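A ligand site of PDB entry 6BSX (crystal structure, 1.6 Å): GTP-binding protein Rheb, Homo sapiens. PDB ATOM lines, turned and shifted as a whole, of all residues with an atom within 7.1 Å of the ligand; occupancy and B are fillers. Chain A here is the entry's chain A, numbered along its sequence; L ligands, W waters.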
ATOM      1  N   LYS A   9       7.025 -16.859  -6.717  1.00  0.00           N
ATOM      2  CA  LYS A   9       5.651 -17.199  -6.337  1.00  0.00           C
ATOM      3  C   LYS A   9       5.615 -18.551  -5.619  1.00  0.00           C
ATOM      4  O   LYS A   9       6.141 -19.571  -6.144  1.00  0.00           O
ATOM      5  CB  LYS A   9       4.734 -17.226  -7.566  1.00  0.00           C
ATOM      6  CG  LYS A   9       3.272 -17.384  -7.257  1.00  0.00           C
ATOM      7  CD  LYS A   9       2.427 -17.164  -8.564  1.00  0.00           C
ATOM      8  CE  LYS A   9       1.993 -15.721  -8.627  1.00  0.00           C
ATOM      9  NZ  LYS A   9       1.193 -15.383  -9.840  1.00  0.00           N
ATOM     10  N   ILE A  10       5.002 -18.563  -4.442  1.00  0.00           N
ATOM     11  CA  ILE A  10       4.894 -19.793  -3.642  1.00  0.00           C
ATOM     12  C   ILE A  10       3.431 -20.120  -3.456  1.00  0.00           C
ATOM     13  O   ILE A  10       2.672 -19.242  -3.046  1.00  0.00           O
ATOM     14  CB  ILE A  10       5.571 -19.600  -2.249  1.00  0.00           C
ATOM     15  CG1 ILE A  10       7.031 -19.137  -2.429  1.00  0.00           C
ATOM     16  CG2 ILE A  10       5.439 -20.859  -1.343  1.00  0.00           C
ATOM     17  CD1 ILE A  10       7.859 -20.159  -3.140  1.00  0.00           C
ATOM     18  N   ALA A  11       3.051 -21.377  -3.699  1.00  0.00           N
ATOM     19  CA  ALA A  11       1.667 -21.810  -3.475  1.00  0.00           C
ATOM     20  C   ALA A  11       1.559 -22.430  -2.081  1.00  0.00           C
ATOM     21  O   ALA A  11       2.417 -23.179  -1.712  1.00  0.00           O
ATOM     22  CB  ALA A  11       1.228 -22.801  -4.507  1.00  0.00           C
ATOM     23  N   ILE A  12       0.506 -22.093  -1.360  1.00  0.00           N
ATOM     24  CA  ILE A  12       0.260 -22.577  -0.013  1.00  0.00           C
ATOM     25  C   ILE A  12      -0.907 -23.548  -0.114  1.00  0.00           C
ATOM     26  O   ILE A  12      -2.016 -23.152  -0.484  1.00  0.00           O
ATOM     27  CB  ILE A  12      -0.073 -21.474   0.945  1.00  0.00           C
ATOM     28  CG1 ILE A  12       1.141 -20.509   0.960  1.00  0.00           C
ATOM     29  CG2 ILE A  12      -0.336 -22.046   2.350  1.00  0.00           C
ATOM     30  CD1 ILE A  12       0.808 -19.133   1.264  1.00  0.00           C
ATOM     31  N   LEU A  13      -0.655 -24.822   0.219  1.00  0.00           N
ATOM     32  CA  LEU A  13      -1.647 -25.872  -0.024  1.00  0.00           C
ATOM     33  C   LEU A  13      -2.014 -26.496   1.305  1.00  0.00           C
ATOM     34  O   LEU A  13      -1.298 -26.303   2.297  1.00  0.00           O
ATOM     35  CB  LEU A  13      -1.078 -26.903  -0.985  1.00  0.00           C
ATOM     36  CG  LEU A  13      -0.459 -26.562  -2.324  1.00  0.00           C
ATOM     37  CD1 LEU A  13       0.035 -27.821  -3.052  1.00  0.00           C
ATOM     38  CD2 LEU A  13      -1.553 -25.838  -3.135  1.00  0.00           C
ATOM     39  N   LYS A  20      -4.131 -21.831   6.449  1.00  0.00           N
ATOM     40  CA  LYS A  20      -3.361 -21.276   5.301  1.00  0.00           C
ATOM     41  C   LYS A  20      -3.557 -19.727   5.187  1.00  0.00           C
ATOM     42  O   LYS A  20      -2.543 -18.950   5.108  1.00  0.00           O
ATOM     43  CB  LYS A  20      -3.748 -21.978   3.992  1.00  0.00           C
ATOM     44  CG  LYS A  20      -3.454 -23.485   3.867  1.00  0.00           C
ATOM     45  CD  LYS A  20      -3.951 -23.968   2.481  1.00  0.00           C
ATOM     46  CE  LYS A  20      -5.414 -23.607   2.275  1.00  0.00           C
ATOM     47  NZ  LYS A  20      -6.407 -24.390   3.143  1.00  0.00           N
ATOM     48  N   THR A  39     -13.423 -19.776   1.100  1.00  0.00           N
ATOM     49  CA  THR A  39     -13.670 -20.240  -0.259  1.00  0.00           C
ATOM     50  C   THR A  39     -12.851 -19.420  -1.279  1.00  0.00           C
ATOM     51  O   THR A  39     -12.818 -19.735  -2.461  1.00  0.00           O
ATOM     52  CB  THR A  39     -15.175 -20.137  -0.672  1.00  0.00           C
ATOM     53  OG1 THR A  39     -15.568 -18.759  -0.847  1.00  0.00           O
ATOM     54  CG2 THR A  39     -16.060 -20.839   0.374  1.00  0.00           C
ATOM     55  N   GLU A  41      -9.368 -17.736  -2.953  1.00  0.00           N
ATOM     56  CA  GLU A  41      -7.983 -17.826  -3.298  1.00  0.00           C
ATOM     57  C   GLU A  41      -7.513 -16.440  -3.738  1.00  0.00           C
ATOM     58  O   GLU A  41      -8.057 -15.852  -4.668  1.00  0.00           O
ATOM     59  CB  GLU A  41      -7.746 -18.885  -4.406  1.00  0.00           C
ATOM     60  CG  GLU A  41      -6.286 -19.016  -4.861  1.00  0.00           C
ATOM     61  CD  GLU A  41      -6.052 -20.203  -5.811  1.00  0.00           C
ATOM     62  OE1 GLU A  41      -6.626 -21.284  -5.577  1.00  0.00           O
ATOM     63  OE2 GLU A  41      -5.280 -20.086  -6.779  1.00  0.00           O
ATOM     64  N   VAL A  60       0.402 -17.525  -2.983  1.00  0.00           N
ATOM     65  CA  VAL A  60      -0.912 -17.933  -3.482  1.00  0.00           C
ATOM     66  C   VAL A  60      -1.595 -18.774  -2.354  1.00  0.00           C
ATOM     67  O   VAL A  60      -1.273 -19.938  -2.141  1.00  0.00           O
ATOM     68  CB  VAL A  60      -0.815 -18.750  -4.790  1.00  0.00           C
ATOM     69  CG1 VAL A  60      -2.235 -19.068  -5.330  1.00  0.00           C
ATOM     70  CG2 VAL A  60       0.062 -18.059  -5.863  1.00  0.00           C
ATOM     71  N   ASP A  61      -2.456 -18.079  -1.617  1.00  0.00           N
ATOM     72  CA  ASP A  61      -3.256 -18.641  -0.518  1.00  0.00           C
ATOM     73  C   ASP A  61      -4.429 -19.391  -1.114  1.00  0.00           C
ATOM     74  O   ASP A  61      -5.505 -18.819  -1.298  1.00  0.00           O
ATOM     75  CB  ASP A  61      -3.711 -17.503   0.409  1.00  0.00           C
ATOM     76  CG  ASP A  61      -4.656 -17.969   1.510  1.00  0.00           C
ATOM     77  OD1 ASP A  61      -4.510 -19.147   1.988  1.00  0.00           O
ATOM     78  OD2 ASP A  61      -5.533 -17.152   1.955  1.00  0.00           O
ATOM     79  N   THR A  62      -4.225 -20.674  -1.416  1.00  0.00           N
ATOM     80  CA  THR A  62      -5.256 -21.483  -2.070  1.00  0.00           C
ATOM     81  C   THR A  62      -6.433 -21.783  -1.148  1.00  0.00           C
ATOM     82  O   THR A  62      -6.283 -21.739   0.088  1.00  0.00           O
ATOM     83  CB  THR A  62      -4.715 -22.828  -2.599  1.00  0.00           C
ATOM     84  OG1 THR A  62      -4.415 -23.696  -1.481  1.00  0.00           O
ATOM     85  CG2 THR A  62      -3.475 -22.628  -3.470  1.00  0.00           C
ATOM     86  N   ALA A  63      -7.612 -22.018  -1.764  1.00  0.00           N
ATOM     87  CA  ALA A  63      -8.834 -22.281  -0.977  1.00  0.00           C
ATOM     88  C   ALA A  63      -8.794 -23.570  -0.200  1.00  0.00           C
ATOM     89  O   ALA A  63      -9.407 -23.651   0.838  1.00  0.00           O
ATOM     90  CB  ALA A  63     -10.105 -22.270  -1.890  1.00  0.00           C
ATOM     91  N   GLY A  64      -8.100 -24.574  -0.710  1.00  0.00           N
ATOM     92  CA  GLY A  64      -7.970 -25.823   0.002  1.00  0.00           C
ATOM     93  C   GLY A  64      -8.093 -27.034  -0.893  1.00  0.00           C
ATOM     94  O   GLY A  64      -8.661 -26.950  -1.998  1.00  0.00           O
ATOM     95  N   GLN A  65      -7.550 -28.167  -0.446  1.00  0.00           N
ATOM     96  CA  GLN A  65      -7.563 -29.376  -1.258  1.00  0.00           C
ATOM     97  C   GLN A  65      -7.982 -30.507  -0.346  1.00  0.00           C
ATOM     98  O   GLN A  65      -7.934 -30.385   0.880  1.00  0.00           O
ATOM     99  CB  GLN A  65      -6.209 -29.706  -1.886  1.00  0.00           C
ATOM    100  CG  GLN A  65      -5.657 -28.651  -2.846  1.00  0.00           C
ATOM    101  CD  GLN A  65      -5.072 -27.434  -2.135  1.00  0.00           C
ATOM    102  OE1 GLN A  65      -4.318 -27.596  -1.179  1.00  0.00           O
ATOM    103  NE2 GLN A  65      -5.431 -26.230  -2.576  1.00  0.00           N
ATOM    104  N   SER A  69      -9.027 -33.659  -4.736  1.00  0.00           N
ATOM    105  CA  SER A  69      -8.479 -32.551  -5.511  1.00  0.00           C
ATOM    106  C   SER A  69      -7.568 -33.008  -6.653  1.00  0.00           C
ATOM    107  O   SER A  69      -6.978 -34.066  -6.549  1.00  0.00           O
ATOM    108  CB  SER A  69      -7.700 -31.631  -4.583  1.00  0.00           C
ATOM    109  OG  SER A  69      -8.566 -30.985  -3.673  1.00  0.00           O
ATOM    110  N   ILE A  70      -7.417 -32.177  -7.696  1.00  0.00           N
ATOM    111  CA  ILE A  70      -6.565 -32.541  -8.831  1.00  0.00           C
ATOM    112  C   ILE A  70      -5.436 -31.566  -9.002  1.00  0.00           C
ATOM    113  O   ILE A  70      -5.528 -30.428  -8.535  1.00  0.00           O
ATOM    114  CB  ILE A  70      -7.374 -32.624 -10.147  1.00  0.00           C
ATOM    115  CG1 ILE A  70      -7.970 -31.270 -10.499  1.00  0.00           C
ATOM    116  CG2 ILE A  70      -8.458 -33.700 -10.017  1.00  0.00           C
ATOM    117  CD1 ILE A  70      -8.971 -31.301 -11.676  1.00  0.00           C
ATOM    118  N   PHE A  71      -4.374 -32.005  -9.663  1.00  0.00           N
ATOM    119  CA  PHE A  71      -3.160 -31.202  -9.808  1.00  0.00           C
ATOM    120  C   PHE A  71      -2.613 -31.299 -11.231  1.00  0.00           C
ATOM    121  O   PHE A  71      -1.545 -31.867 -11.455  1.00  0.00           O
ATOM    122  CB  PHE A  71      -2.112 -31.665  -8.809  1.00  0.00           C
ATOM    123  CG  PHE A  71      -2.491 -31.364  -7.381  1.00  0.00           C
ATOM    124  CD1 PHE A  71      -3.255 -32.250  -6.637  1.00  0.00           C
ATOM    125  CD2 PHE A  71      -2.105 -30.179  -6.789  1.00  0.00           C
ATOM    126  CE1 PHE A  71      -3.627 -31.951  -5.345  1.00  0.00           C
ATOM    127  CE2 PHE A  71      -2.455 -29.888  -5.488  1.00  0.00           C
ATOM    128  CZ  PHE A  71      -3.212 -30.772  -4.774  1.00  0.00           C
ATOM    129  N   PRO A  72      -3.339 -30.713 -12.185  1.00  0.00           N
ATOM    130  CA  PRO A  72      -2.865 -30.607 -13.561  1.00  0.00           C
ATOM    131  C   PRO A  72      -1.610 -29.766 -13.663  1.00  0.00           C
ATOM    132  O   PRO A  72      -1.512 -28.792 -12.922  1.00  0.00           O
ATOM    133  CB  PRO A  72      -4.011 -29.902 -14.296  1.00  0.00           C
ATOM    134  CG  PRO A  72      -5.168 -29.853 -13.354  1.00  0.00           C
ATOM    135  CD  PRO A  72      -4.630 -30.014 -11.970  1.00  0.00           C
ATOM    136  N   THR A  74      -0.804 -27.559 -15.649  1.00  0.00           N
ATOM    137  CA  THR A  74      -1.294 -26.196 -15.819  1.00  0.00           C
ATOM    138  C   THR A  74      -1.245 -25.357 -14.518  1.00  0.00           C
ATOM    139  O   THR A  74      -0.871 -24.173 -14.541  1.00  0.00           O
ATOM    140  CB  THR A  74      -2.747 -26.195 -16.332  1.00  0.00           C
ATOM    141  N   TYR A  75      -1.632 -25.971 -13.404  1.00  0.00           N
ATOM    142  CA  TYR A  75      -1.640 -25.278 -12.099  1.00  0.00           C
ATOM    143  C   TYR A  75      -0.225 -24.866 -11.639  1.00  0.00           C
ATOM    144  O   TYR A  75      -0.086 -23.976 -10.800  1.00  0.00           O
ATOM    145  CB  TYR A  75      -2.268 -26.169 -11.007  1.00  0.00           C
ATOM    146  CG  TYR A  75      -3.770 -26.437 -11.116  1.00  0.00           C
ATOM    147  CD1 TYR A  75      -4.508 -26.013 -12.222  1.00  0.00           C
ATOM    148  CD2 TYR A  75      -4.452 -27.125 -10.105  1.00  0.00           C
ATOM    149  CE1 TYR A  75      -5.872 -26.264 -12.323  1.00  0.00           C
ATOM    150  CE2 TYR A  75      -5.825 -27.393 -10.196  1.00  0.00           C
ATOM    151  CZ  TYR A  75      -6.532 -26.960 -11.305  1.00  0.00           C
ATOM    152  OH  TYR A  75      -7.886 -27.220 -11.404  1.00  0.00           O
ATOM    153  N   SER A  76       0.799 -25.530 -12.155  1.00  0.00           N
ATOM    154  CA  SER A  76       2.163 -25.289 -11.709  1.00  0.00           C
ATOM    155  C   SER A  76       2.839 -24.130 -12.438  1.00  0.00           C
ATOM    156  O   SER A  76       4.007 -23.851 -12.195  1.00  0.00           O
ATOM    157  CB  SER A  76       3.013 -26.541 -11.888  1.00  0.00           C
ATOM    158  N   ILE A  77       2.133 -23.468 -13.341  1.00  0.00           N
ATOM    159  CA  ILE A  77       2.788 -22.453 -14.168  1.00  0.00           C
ATOM    160  C   ILE A  77       3.140 -21.219 -13.346  1.00  0.00           C
ATOM    161  O   ILE A  77       2.293 -20.639 -12.677  1.00  0.00           O
ATOM    162  CB  ILE A  77       1.937 -22.043 -15.363  1.00  0.00           C
ATOM    163  CG1 ILE A  77       1.658 -23.262 -16.239  1.00  0.00           C
ATOM    164  CG2 ILE A  77       2.652 -20.960 -16.195  1.00  0.00           C
ATOM    165  CD1 ILE A  77       2.908 -23.854 -16.814  1.00  0.00           C
ATOM    166  N   ILE A  79       4.930 -21.173 -10.706  1.00  0.00           N
ATOM    167  CA  ILE A  79       5.135 -21.444  -9.276  1.00  0.00           C
ATOM    168  C   ILE A  79       6.555 -21.873  -8.971  1.00  0.00           C
ATOM    169  O   ILE A  79       7.070 -22.835  -9.563  1.00  0.00           O
ATOM    170  CB  ILE A  79       4.166 -22.519  -8.740  1.00  0.00           C
ATOM    171  CG1 ILE A  79       2.729 -22.049  -8.922  1.00  0.00           C
ATOM    172  CG2 ILE A  79       4.448 -22.816  -7.257  1.00  0.00           C
ATOM    173  CD1 ILE A  79       2.337 -20.864  -8.090  1.00  0.00           C
ATOM    174  N   TYR A  82       6.405 -24.676  -3.052  1.00  0.00           N
ATOM    175  CA  TYR A  82       5.174 -25.117  -2.401  1.00  0.00           C
ATOM    176  C   TYR A  82       5.327 -25.227  -0.881  1.00  0.00           C
ATOM    177  O   TYR A  82       6.323 -25.744  -0.381  1.00  0.00           O
ATOM    178  CB  TYR A  82       4.766 -26.477  -2.963  1.00  0.00           C
ATOM    179  CG  TYR A  82       4.447 -26.402  -4.431  1.00  0.00           C
ATOM    180  CD1 TYR A  82       5.468 -26.518  -5.395  1.00  0.00           C
ATOM    181  CD2 TYR A  82       3.161 -26.169  -4.871  1.00  0.00           C
ATOM    182  CE1 TYR A  82       5.205 -26.448  -6.734  1.00  0.00           C
ATOM    183  CE2 TYR A  82       2.900 -26.064  -6.244  1.00  0.00           C
ATOM    184  CZ  TYR A  82       3.920 -26.213  -7.160  1.00  0.00           C
ATOM    185  OH  TYR A  82       3.656 -26.121  -8.538  1.00  0.00           O
ATOM    186  N   LEU A 104       1.053 -33.815  -5.910  1.00  0.00           N
ATOM    187  CA  LEU A 104       1.964 -32.700  -6.257  1.00  0.00           C
ATOM    188  C   LEU A 104       3.192 -33.199  -7.005  1.00  0.00           C
ATOM    189  O   LEU A 104       3.586 -32.634  -8.031  1.00  0.00           O
ATOM    190  CB  LEU A 104       2.371 -31.954  -4.991  1.00  0.00           C
ATOM    191  CG  LEU A 104       3.265 -30.737  -5.197  1.00  0.00           C
ATOM    192  CD1 LEU A 104       2.551 -29.781  -6.141  1.00  0.00           C
ATOM    193  CD2 LEU A 104       3.463 -30.097  -3.873  1.00  0.00           C
ATOM    194  N   MET A 107       2.627 -33.982 -10.448  1.00  0.00           N
ATOM    195  CA  MET A 107       2.489 -32.805 -11.269  1.00  0.00           C
ATOM    196  C   MET A 107       3.855 -32.229 -11.616  1.00  0.00           C
ATOM    197  O   MET A 107       4.121 -31.969 -12.790  1.00  0.00           O
ATOM    198  CB  MET A 107       1.639 -31.746 -10.564  1.00  0.00           C
ATOM    199  CG  MET A 107       1.469 -30.432 -11.386  1.00  0.00           C
ATOM    200  SD  MET A 107       0.584 -29.176 -10.454  1.00  0.00           S
ATOM    201  CE  MET A 107       1.843 -28.716  -9.282  1.00  0.00           C
HETATM  202  C1  LIG L   1      -4.482 -24.219  -6.432  1.00  0.00           C
HETATM  203  C2  LIG L   1      -0.731 -26.178  -7.578  1.00  0.00           C
HETATM  204  C3  LIG L   1      -2.160 -25.423  -7.139  1.00  0.00           C
HETATM  205  C4  LIG L   1      -3.247 -26.237  -6.888  1.00  0.00           C
HETATM  206  C5  LIG L   1      -4.430 -25.610  -6.520  1.00  0.00           C
HETATM  207  N1  LIG L   1      -5.690 -26.160  -6.230  1.00  0.00           N
HETATM  208  C6  LIG L   1      -6.467 -25.110  -5.941  1.00  0.00           C
HETATM  209  C7  LIG L   1      -7.918 -25.081  -5.504  1.00  0.00           C
HETATM  210  O1  LIG L   1      -7.948 -24.437  -4.198  1.00  0.00           O
HETATM  211  N2  LIG L   1      -5.776 -23.897  -6.055  1.00  0.00           N
HETATM  212  C8  LIG L   1      -3.393 -23.395  -6.693  1.00  0.00           C
HETATM  213  C9  LIG L   1      -2.238 -24.015  -7.025  1.00  0.00           C
HETATM  214  C10 LIG L   1      -0.915 -22.980  -7.347  1.00  0.00           C
HETATM  215  O   HOH W   1      -6.238 -28.645  -6.698  1.00  0.00           O
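An oxygen (O1) of the ligand lies within hydrogen-bond range of the side-chain amide nitrogen (NE2) of Gln 65 (3.5 Å). N of Ala 63 is in hydrogen-bond range of O1 of the ligand (3.4 Å). The backbone NH of Gly 64 sits at hydrogen-bond distance from an oxygen (O1) of the ligand. The side-chain carboxylate of Glu 41 sits at hydrogen-bond distance from a nitrogen (N2) of the ligand (2.8 Å). The backbone carbonyl oxygen of Gly 64 lies within hydrogen-bond range of an oxygen (O1) of the ligand.
OG1 of Thr 62 sits at hydrogen-bond distance from NE2 of Gln 65 (2.9 Å). OG1 of Thr 62 is in hydrogen-bond range of O of Ile 12.
CB of Ala 11 touches C10 of the ligand, at 3.6 Å. Thr 62 touches the ligand. CE2 of Phe 71 touches C4 of the ligand, at 3.99 Å. CD2 of Tyr 75 touches C4 of the ligand, at 3.5 Å. Ile 79 touches the ligand (CD1 to C10, 3.95 Å). Tyr 82 touches the ligand. CE of Met 107 touches C2 of the ligand, at 3.996 Å. Hydrophobic or aromatic side chains within 4 Å of the ligand: Ala 11, Ala 63, Phe 71, Tyr 75, Ile 79, Tyr 82 and Met 107. The nearest printed residue that does not touch the ligand is Leu 13 (4.1 Å).
Water W1 bridges N1 of the ligand (2.6 Å) and O of Ile 70 (2.7 Å).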
